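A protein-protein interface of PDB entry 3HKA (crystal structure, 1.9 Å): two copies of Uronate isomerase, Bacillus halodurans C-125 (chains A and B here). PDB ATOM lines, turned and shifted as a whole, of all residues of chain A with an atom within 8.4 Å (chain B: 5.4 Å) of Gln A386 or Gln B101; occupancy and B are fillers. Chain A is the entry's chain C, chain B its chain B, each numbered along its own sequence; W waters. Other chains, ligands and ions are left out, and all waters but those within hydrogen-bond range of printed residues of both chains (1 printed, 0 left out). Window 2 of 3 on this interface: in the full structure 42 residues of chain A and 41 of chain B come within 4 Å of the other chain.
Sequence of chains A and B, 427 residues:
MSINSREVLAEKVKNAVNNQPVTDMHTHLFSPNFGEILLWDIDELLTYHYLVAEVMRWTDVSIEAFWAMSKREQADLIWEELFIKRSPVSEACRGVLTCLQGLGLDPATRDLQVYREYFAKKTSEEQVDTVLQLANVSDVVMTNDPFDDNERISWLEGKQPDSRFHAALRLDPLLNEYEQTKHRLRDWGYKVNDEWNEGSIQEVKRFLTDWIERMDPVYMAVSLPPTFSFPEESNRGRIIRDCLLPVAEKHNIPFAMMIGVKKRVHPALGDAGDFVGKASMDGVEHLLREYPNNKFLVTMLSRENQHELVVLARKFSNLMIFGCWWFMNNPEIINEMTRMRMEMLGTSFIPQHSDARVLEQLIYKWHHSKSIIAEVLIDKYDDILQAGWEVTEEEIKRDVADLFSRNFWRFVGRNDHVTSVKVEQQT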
ATOM      1  N   ASN A   4       0.611  -4.067 -16.185  1.00  0.00           N
ATOM      2  CA  ASN A   4       0.498  -3.795 -14.755  1.00  0.00           C
ATOM      3  C   ASN A   4      -0.927  -3.502 -14.286  1.00  0.00           C
ATOM      4  O   ASN A   4      -1.483  -4.241 -13.474  1.00  0.00           O
ATOM      5  CB  ASN A   4       1.414  -2.621 -14.387  1.00  0.00           C
ATOM      6  CG  ASN A   4       1.461  -2.353 -12.889  1.00  0.00           C
ATOM      7  OD1 ASN A   4       0.445  -2.033 -12.267  1.00  0.00           O
ATOM      8  ND2 ASN A   4       2.649  -2.482 -12.303  1.00  0.00           N
ATOM      9  N   SER A   5      -1.515  -2.423 -14.796  1.00  0.00           N
ATOM     10  CA  SER A   5      -2.865  -2.033 -14.398  1.00  0.00           C
ATOM     11  C   SER A   5      -3.919  -2.305 -15.465  1.00  0.00           C
ATOM     12  O   SER A   5      -3.601  -2.570 -16.625  1.00  0.00           O
ATOM     13  CB  SER A   5      -2.895  -0.545 -14.046  1.00  0.00           C
ATOM     14  OG  SER A   5      -2.622   0.248 -15.190  1.00  0.00           O
ATOM     15  N   ARG A   6      -5.182  -2.230 -15.058  1.00  0.00           N
ATOM     16  CA  ARG A   6      -6.292  -2.447 -15.972  1.00  0.00           C
ATOM     17  C   ARG A   6      -6.224  -1.368 -17.046  1.00  0.00           C
ATOM     18  O   ARG A   6      -6.593  -1.592 -18.196  1.00  0.00           O
ATOM     19  CB  ARG A   6      -7.618  -2.359 -15.213  1.00  0.00           C
ATOM     20  CG  ARG A   6      -8.850  -2.692 -16.043  1.00  0.00           C
ATOM     21  CD  ARG A   6     -10.084  -2.764 -15.154  1.00  0.00           C
ATOM     22  NE  ARG A   6     -11.271  -3.235 -15.863  1.00  0.00           N
ATOM     23  CZ  ARG A   6     -11.833  -2.595 -16.881  1.00  0.00           C
ATOM     24  NH1 ARG A   6     -11.316  -1.454 -17.316  1.00  0.00           N
ATOM     25  NH2 ARG A   6     -12.918  -3.091 -17.461  1.00  0.00           N
ATOM     26  N   LEU A   9      -3.803  -2.482 -19.501  1.00  0.00           N
ATOM     27  CA  LEU A   9      -4.431  -3.615 -20.164  1.00  0.00           C
ATOM     28  C   LEU A   9      -5.386  -3.134 -21.249  1.00  0.00           C
ATOM     29  O   LEU A   9      -5.317  -3.580 -22.395  1.00  0.00           O
ATOM     30  CB  LEU A   9      -5.199  -4.450 -19.140  1.00  0.00           C
ATOM     31  CG  LEU A   9      -5.902  -5.717 -19.627  1.00  0.00           C
ATOM     32  CD1 LEU A   9      -4.881  -6.712 -20.149  1.00  0.00           C
ATOM     33  CD2 LEU A   9      -6.690  -6.317 -18.480  1.00  0.00           C
ATOM     34  N   ASP A 379     -12.160  -7.035 -19.322  1.00  0.00           N
ATOM     35  CA  ASP A 379     -12.678  -7.586 -18.072  1.00  0.00           C
ATOM     36  C   ASP A 379     -12.145  -8.990 -17.811  1.00  0.00           C
ATOM     37  O   ASP A 379     -11.739  -9.309 -16.693  1.00  0.00           O
ATOM     38  CB  ASP A 379     -14.209  -7.650 -18.081  1.00  0.00           C
ATOM     39  CG  ASP A 379     -14.863  -6.323 -17.726  1.00  0.00           C
ATOM     40  OD1 ASP A 379     -14.265  -5.541 -16.956  1.00  0.00           O
ATOM     41  OD2 ASP A 379     -15.991  -6.078 -18.203  1.00  0.00           O
ATOM     42  N   LYS A 380     -12.168  -9.839 -18.835  1.00  0.00           N
ATOM     43  CA  LYS A 380     -11.691 -11.205 -18.669  1.00  0.00           C
ATOM     44  C   LYS A 380     -10.186 -11.282 -18.431  1.00  0.00           C
ATOM     45  O   LYS A 380      -9.728 -12.072 -17.607  1.00  0.00           O
ATOM     46  CB  LYS A 380     -12.093 -12.067 -19.870  1.00  0.00           C
ATOM     47  CG  LYS A 380     -13.493 -12.665 -19.735  1.00  0.00           C
ATOM     48  CD  LYS A 380     -14.539 -11.578 -19.582  1.00  0.00           C
ATOM     49  CE  LYS A 380     -15.919 -12.163 -19.345  1.00  0.00           C
ATOM     50  NZ  LYS A 380     -15.994 -12.886 -18.050  1.00  0.00           N
ATOM     51  N   TYR A 381      -9.417 -10.472 -19.150  1.00  0.00           N
ATOM     52  CA  TYR A 381      -7.974 -10.466 -18.943  1.00  0.00           C
ATOM     53  C   TYR A 381      -7.685  -9.915 -17.546  1.00  0.00           C
ATOM     54  O   TYR A 381      -6.846 -10.448 -16.822  1.00  0.00           O
ATOM     55  CB  TYR A 381      -7.270  -9.599 -19.989  1.00  0.00           C
ATOM     56  CG  TYR A 381      -7.099 -10.251 -21.349  1.00  0.00           C
ATOM     57  CD1 TYR A 381      -6.540 -11.524 -21.476  1.00  0.00           C
ATOM     58  CD2 TYR A 381      -7.440  -9.566 -22.512  1.00  0.00           C
ATOM     59  CE1 TYR A 381      -6.319 -12.096 -22.736  1.00  0.00           C
ATOM     60  CE2 TYR A 381      -7.223 -10.123 -23.770  1.00  0.00           C
ATOM     61  CZ  TYR A 381      -6.663 -11.383 -23.875  1.00  0.00           C
ATOM     62  OH  TYR A 381      -6.434 -11.910 -25.124  1.00  0.00           O
ATOM     63  N   ASP A 382      -8.390  -8.855 -17.160  1.00  0.00           N
ATOM     64  CA  ASP A 382      -8.180  -8.259 -15.843  1.00  0.00           C
ATOM     65  C   ASP A 382      -8.475  -9.254 -14.723  1.00  0.00           C
ATOM     66  O   ASP A 382      -7.743  -9.316 -13.731  1.00  0.00           O
ATOM     67  CB  ASP A 382      -9.051  -7.005 -15.668  1.00  0.00           C
ATOM     68  CG  ASP A 382      -8.646  -6.179 -14.449  1.00  0.00           C
ATOM     69  OD1 ASP A 382      -7.433  -5.967 -14.258  1.00  0.00           O
ATOM     70  OD2 ASP A 382      -9.531  -5.733 -13.690  1.00  0.00           O
ATOM     71  N   ASP A 383      -9.538 -10.043 -14.874  1.00  0.00           N
ATOM     72  CA  ASP A 383      -9.871 -11.022 -13.841  1.00  0.00           C
ATOM     73  C   ASP A 383      -8.756 -12.037 -13.611  1.00  0.00           C
ATOM     74  O   ASP A 383      -8.503 -12.432 -12.471  1.00  0.00           O
ATOM     75  CB  ASP A 383     -11.174 -11.766 -14.169  1.00  0.00           C
ATOM     76  CG  ASP A 383     -12.408 -10.934 -13.885  1.00  0.00           C
ATOM     77  OD1 ASP A 383     -12.354 -10.075 -12.974  1.00  0.00           O
ATOM     78  OD2 ASP A 383     -13.439 -11.146 -14.559  1.00  0.00           O
ATOM     79  N   ILE A 384      -8.092 -12.477 -14.677  1.00  0.00           N
ATOM     80  CA  ILE A 384      -7.016 -13.447 -14.494  1.00  0.00           C
ATOM     81  C   ILE A 384      -5.740 -12.750 -14.022  1.00  0.00           C
ATOM     82  O   ILE A 384      -4.903 -13.362 -13.356  1.00  0.00           O
ATOM     83  CB  ILE A 384      -6.740 -14.274 -15.781  1.00  0.00           C
ATOM     84  CG1 ILE A 384      -6.541 -13.357 -16.984  1.00  0.00           C
ATOM     85  CG2 ILE A 384      -7.896 -15.245 -16.028  1.00  0.00           C
ATOM     86  CD1 ILE A 384      -6.168 -14.109 -18.248  1.00  0.00           C
ATOM     87  N   LEU A 385      -5.595 -11.471 -14.367  1.00  0.00           N
ATOM     88  CA  LEU A 385      -4.437 -10.698 -13.926  1.00  0.00           C
ATOM     89  C   LEU A 385      -4.543 -10.570 -12.411  1.00  0.00           C
ATOM     90  O   LEU A 385      -3.544 -10.666 -11.699  1.00  0.00           O
ATOM     91  CB  LEU A 385      -4.438  -9.300 -14.550  1.00  0.00           C
ATOM     92  CG  LEU A 385      -3.860  -9.152 -15.960  1.00  0.00           C
ATOM     93  CD1 LEU A 385      -3.990  -7.705 -16.415  1.00  0.00           C
ATOM     94  CD2 LEU A 385      -2.398  -9.572 -15.964  1.00  0.00           C
ATOM     95  N   GLN A 386      -5.767 -10.355 -11.931  1.00  0.00           N
ATOM     96  CA  GLN A 386      -6.029 -10.226 -10.502  1.00  0.00           C
ATOM     97  C   GLN A 386      -5.817 -11.561  -9.807  1.00  0.00           C
ATOM     98  O   GLN A 386      -5.659 -11.618  -8.589  1.00  0.00           O
ATOM     99  CB  GLN A 386      -7.462  -9.746 -10.255  1.00  0.00           C
ATOM    100  CG  GLN A 386      -7.698  -8.288 -10.600  1.00  0.00           C
ATOM    101  CD  GLN A 386      -6.746  -7.360  -9.859  1.00  0.00           C
ATOM    102  OE1 GLN A 386      -6.655  -7.395  -8.629  1.00  0.00           O
ATOM    103  NE2 GLN A 386      -6.032  -6.523 -10.608  1.00  0.00           N
ATOM    104  N   ALA A 387      -5.824 -12.636 -10.585  1.00  0.00           N
ATOM    105  CA  ALA A 387      -5.616 -13.966 -10.031  1.00  0.00           C
ATOM    106  C   ALA A 387      -4.120 -14.268  -9.987  1.00  0.00           C
ATOM    107  O   ALA A 387      -3.699 -15.291  -9.445  1.00  0.00           O
ATOM    108  CB  ALA A 387      -6.342 -15.010 -10.878  1.00  0.00           C
ATOM    109  N   GLY A 388      -3.319 -13.375 -10.564  1.00  0.00           N
ATOM    110  CA  GLY A 388      -1.879 -13.569 -10.558  1.00  0.00           C
ATOM    111  C   GLY A 388      -1.267 -13.921 -11.901  1.00  0.00           C
ATOM    112  O   GLY A 388      -0.046 -13.953 -12.039  1.00  0.00           O
ATOM    113  N   TRP A 389      -2.110 -14.186 -12.895  1.00  0.00           N
ATOM    114  CA  TRP A 389      -1.635 -14.537 -14.228  1.00  0.00           C
ATOM    115  C   TRP A 389      -1.103 -13.298 -14.932  1.00  0.00           C
ATOM    116  O   TRP A 389      -1.599 -12.195 -14.721  1.00  0.00           O
ATOM    117  CB  TRP A 389      -2.781 -15.154 -15.041  1.00  0.00           C
ATOM    118  CG  TRP A 389      -2.374 -15.715 -16.375  1.00  0.00           C
ATOM    119  CD1 TRP A 389      -2.415 -15.079 -17.585  1.00  0.00           C
ATOM    120  CD2 TRP A 389      -1.893 -17.039 -16.633  1.00  0.00           C
ATOM    121  NE1 TRP A 389      -1.993 -15.928 -18.582  1.00  0.00           N
ATOM    122  CE2 TRP A 389      -1.666 -17.138 -18.025  1.00  0.00           C
ATOM    123  CE3 TRP A 389      -1.633 -18.153 -15.825  1.00  0.00           C
ATOM    124  CZ2 TRP A 389      -1.192 -18.308 -18.627  1.00  0.00           C
ATOM    125  CZ3 TRP A 389      -1.159 -19.318 -16.424  1.00  0.00           C
ATOM    126  CH2 TRP A 389      -0.945 -19.385 -17.812  1.00  0.00           C
ATOM    127  N   GLU A 390      -0.082 -13.478 -15.759  1.00  0.00           N
ATOM    128  CA  GLU A 390       0.493 -12.359 -16.486  1.00  0.00           C
ATOM    129  C   GLU A 390       0.363 -12.557 -17.991  1.00  0.00           C
ATOM    130  O   GLU A 390       1.057 -13.382 -18.584  1.00  0.00           O
ATOM    131  CB  GLU A 390       1.961 -12.183 -16.097  1.00  0.00           C
ATOM    132  CG  GLU A 390       2.153 -11.841 -14.629  1.00  0.00           C
ATOM    133  CD  GLU A 390       3.608 -11.624 -14.268  1.00  0.00           C
ATOM    134  OE1 GLU A 390       3.895 -11.350 -13.082  1.00  0.00           O
ATOM    135  OE2 GLU A 390       4.466 -11.725 -15.173  1.00  0.00           O
ATOM    136  N   VAL A 391      -0.535 -11.794 -18.601  1.00  0.00           N
ATOM    137  CA  VAL A 391      -0.768 -11.882 -20.035  1.00  0.00           C
ATOM    138  C   VAL A 391       0.172 -10.959 -20.797  1.00  0.00           C
ATOM    139  O   VAL A 391       0.314  -9.786 -20.453  1.00  0.00           O
ATOM    140  CB  VAL A 391      -2.214 -11.482 -20.391  1.00  0.00           C
ATOM    141  CG1 VAL A 391      -2.454 -11.672 -21.879  1.00  0.00           C
ATOM    142  CG2 VAL A 391      -3.197 -12.302 -19.577  1.00  0.00           C
ATOM    143  N   VAL B  96      -9.178 -21.975 -11.731  1.00  0.00           N
ATOM    144  CA  VAL B  96      -8.001 -22.761 -11.376  1.00  0.00           C
ATOM    145  C   VAL B  96      -6.916 -21.818 -10.856  1.00  0.00           C
ATOM    146  O   VAL B  96      -6.311 -22.069  -9.812  1.00  0.00           O
ATOM    147  CB  VAL B  96      -7.455 -23.548 -12.592  1.00  0.00           C
ATOM    148  CG1 VAL B  96      -6.125 -24.217 -12.232  1.00  0.00           C
ATOM    149  CG2 VAL B  96      -8.473 -24.600 -13.024  1.00  0.00           C
ATOM    150  N   LEU B  97      -6.684 -20.729 -11.583  1.00  0.00           N
ATOM    151  CA  LEU B  97      -5.677 -19.746 -11.193  1.00  0.00           C
ATOM    152  C   LEU B  97      -6.003 -19.135  -9.831  1.00  0.00           C
ATOM    153  O   LEU B  97      -5.115 -18.954  -8.993  1.00  0.00           O
ATOM    154  CB  LEU B  97      -5.583 -18.637 -12.246  1.00  0.00           C
ATOM    155  CG  LEU B  97      -5.277 -19.071 -13.683  1.00  0.00           C
ATOM    156  CD1 LEU B  97      -5.199 -17.844 -14.578  1.00  0.00           C
ATOM    157  CD2 LEU B  97      -3.971 -19.847 -13.725  1.00  0.00           C
ATOM    158  N   THR B  98      -7.275 -18.818  -9.612  1.00  0.00           N
ATOM    159  CA  THR B  98      -7.703 -18.237  -8.344  1.00  0.00           C
ATOM    160  C   THR B  98      -7.373 -19.172  -7.183  1.00  0.00           C
ATOM    161  O   THR B  98      -7.003 -18.714  -6.102  1.00  0.00           O
ATOM    162  CB  THR B  98      -9.221 -17.919  -8.356  1.00  0.00           C
ATOM    163  OG1 THR B  98      -9.464 -16.801  -9.223  1.00  0.00           O
ATOM    164  CG2 THR B  98      -9.721 -17.577  -6.954  1.00  0.00           C
ATOM    165  N   CYS B  99      -7.495 -20.479  -7.403  1.00  0.00           N
ATOM    166  CA  CYS B  99      -7.184 -21.452  -6.362  1.00  0.00           C
ATOM    167  C   CYS B  99      -5.684 -21.445  -6.054  1.00  0.00           C
ATOM    168  O   CYS B  99      -5.278 -21.404  -4.888  1.00  0.00           O
ATOM    169  CB  CYS B  99      -7.589 -22.863  -6.794  1.00  0.00           C
ATOM    170  SG  CYS B  99      -9.371 -23.143  -6.956  1.00  0.00           S
ATOM    171  N   LEU B 100      -4.871 -21.501  -7.105  1.00  0.00           N
ATOM    172  CA  LEU B 100      -3.421 -21.510  -6.951  1.00  0.00           C
ATOM    173  C   LEU B 100      -2.970 -20.307  -6.139  1.00  0.00           C
ATOM    174  O   LEU B 100      -2.212 -20.443  -5.176  1.00  0.00           O
ATOM    175  CB  LEU B 100      -2.738 -21.479  -8.321  1.00  0.00           C
ATOM    176  CG  LEU B 100      -2.909 -22.700  -9.227  1.00  0.00           C
ATOM    177  CD1 LEU B 100      -2.364 -22.381 -10.611  1.00  0.00           C
ATOM    178  CD2 LEU B 100      -2.189 -23.895  -8.627  1.00  0.00           C
ATOM    179  N   GLN B 101      -3.443 -19.131  -6.535  1.00  0.00           N
ATOM    180  CA  GLN B 101      -3.088 -17.899  -5.851  1.00  0.00           C
ATOM    181  C   GLN B 101      -3.478 -17.945  -4.380  1.00  0.00           C
ATOM    182  O   GLN B 101      -2.691 -17.580  -3.506  1.00  0.00           O
ATOM    183  CB  GLN B 101      -3.771 -16.706  -6.519  1.00  0.00           C
ATOM    184  CG  GLN B 101      -3.353 -15.369  -5.928  1.00  0.00           C
ATOM    185  CD  GLN B 101      -4.054 -14.197  -6.572  1.00  0.00           C
ATOM    186  OE1 GLN B 101      -5.265 -14.024  -6.419  1.00  0.00           O
ATOM    187  NE2 GLN B 101      -3.299 -13.383  -7.304  1.00  0.00           N
ATOM    188  N   GLY B 102      -4.700 -18.392  -4.112  1.00  0.00           N
ATOM    189  CA  GLY B 102      -5.168 -18.471  -2.742  1.00  0.00           C
ATOM    190  C   GLY B 102      -4.312 -19.371  -1.870  1.00  0.00           C
ATOM    191  O   GLY B 102      -4.190 -19.143  -0.666  1.00  0.00           O
ATOM    192  N   LEU B 103      -3.716 -20.391  -2.478  1.00  0.00           N
ATOM    193  CA  LEU B 103      -2.876 -21.338  -1.754  1.00  0.00           C
ATOM    194  C   LEU B 103      -1.448 -20.843  -1.553  1.00  0.00           C
ATOM    195  O   LEU B 103      -0.638 -21.510  -0.906  1.00  0.00           O
ATOM    196  CB  LEU B 103      -2.843 -22.674  -2.496  1.00  0.00           C
ATOM    197  CG  LEU B 103      -4.136 -23.488  -2.520  1.00  0.00           C
ATOM    198  CD1 LEU B 103      -3.978 -24.649  -3.483  1.00  0.00           C
ATOM    199  CD2 LEU B 103      -4.455 -23.988  -1.119  1.00  0.00           C
ATOM    200  N   GLY B 104      -1.133 -19.681  -2.112  1.00  0.00           N
ATOM    201  CA  GLY B 104       0.206 -19.144  -1.963  1.00  0.00           C
ATOM    202  C   GLY B 104       1.091 -19.402  -3.166  1.00  0.00           C
ATOM    203  O   GLY B 104       2.233 -18.941  -3.213  1.00  0.00           O
ATOM    204  N   LEU B 105       0.576 -20.147  -4.139  1.00  0.00           N
ATOM    205  CA  LEU B 105       1.343 -20.436  -5.341  1.00  0.00           C
ATOM    206  C   LEU B 105       1.205 -19.213  -6.238  1.00  0.00           C
ATOM    207  O   LEU B 105       0.288 -18.413  -6.055  1.00  0.00           O
ATOM    208  CB  LEU B 105       0.800 -21.695  -6.023  1.00  0.00           C
ATOM    209  CG  LEU B 105       0.725 -22.917  -5.099  1.00  0.00           C
ATOM    210  CD1 LEU B 105       0.170 -24.109  -5.857  1.00  0.00           C
ATOM    211  CD2 LEU B 105       2.111 -23.235  -4.547  1.00  0.00           C
ATOM    212  N   PRO B 107       0.649 -17.925 -10.058  1.00  0.00           N
ATOM    213  CA  PRO B 107       0.286 -18.165 -11.459  1.00  0.00           C
ATOM    214  C   PRO B 107       1.203 -17.444 -12.442  1.00  0.00           C
ATOM    215  O   PRO B 107       1.337 -17.847 -13.596  1.00  0.00           O
ATOM    216  CB  PRO B 107      -1.149 -17.655 -11.526  1.00  0.00           C
ATOM    217  CG  PRO B 107      -1.672 -17.992 -10.169  1.00  0.00           C
ATOM    218  CD  PRO B 107      -0.537 -17.529  -9.279  1.00  0.00           C
HETATM  219  O   HOH W   1       1.314 -16.170 -15.935  1.00  0.00           O
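O of Ala A387 sits at hydrogen-bond distance from NE2 of Gln B101, 2.9 Å away. NE2 of Gln B101 sits close to N of Gly A388, at 3.3 Å. The backbone carbonyl oxygen (O) of Gln A386 sits at hydrogen-bond distance from the side-chain amide nitrogen (NE2) of Gln B101 (3.2 Å).
N of Trp A389 is in hydrogen-bond range of O of Ile A384 (2.9 Å).
Among the printed residues, pairs that only touch across the chains: Ala A387 with Leu B97, Ala A387 with Thr B98, Ala A387 with Pro B107, Gly A388 with Pro B107, Trp A389 with Leu B97 and Trp A389 with Pro B107.
Of chain B, only Gln B101 comes within 4 Å of Gln A386. Printed residues of chain B within 4 Å of Gly A388: Gln B101 (3.3 Å) and Pro B107 (3.7 Å). Printed residues of chain A within 4 Å of Leu B97: Ala A387 and Trp A389. Of the printed residues of chain A, Thr B98 touches Ala A387. Gln B101 touches just these residues of chain A: Gln A386 (3.2 Å), Ala A387 (2.9 Å) and Gly A388 (3.3 Å). Gly B102 touches none of the printed residues of chain A. Printed residues of chain A within 4 Å of Pro B107: Ala A387, Gly A388 and Trp A389. The nearest residue of chain A that does not touch Gln B101 is Leu A385 (5.2 Å). The nearest printed residue of chain A that does not touch Pro B107 is Glu A390 (5.1 Å).
Of the 11 printed residues of chain B, 4 touch a printed residue of chain A.
No position is printed for both chains.
Water W1 bridges the backbone carbonyl oxygen of Pro B107 and the backbone NH of Glu A390.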
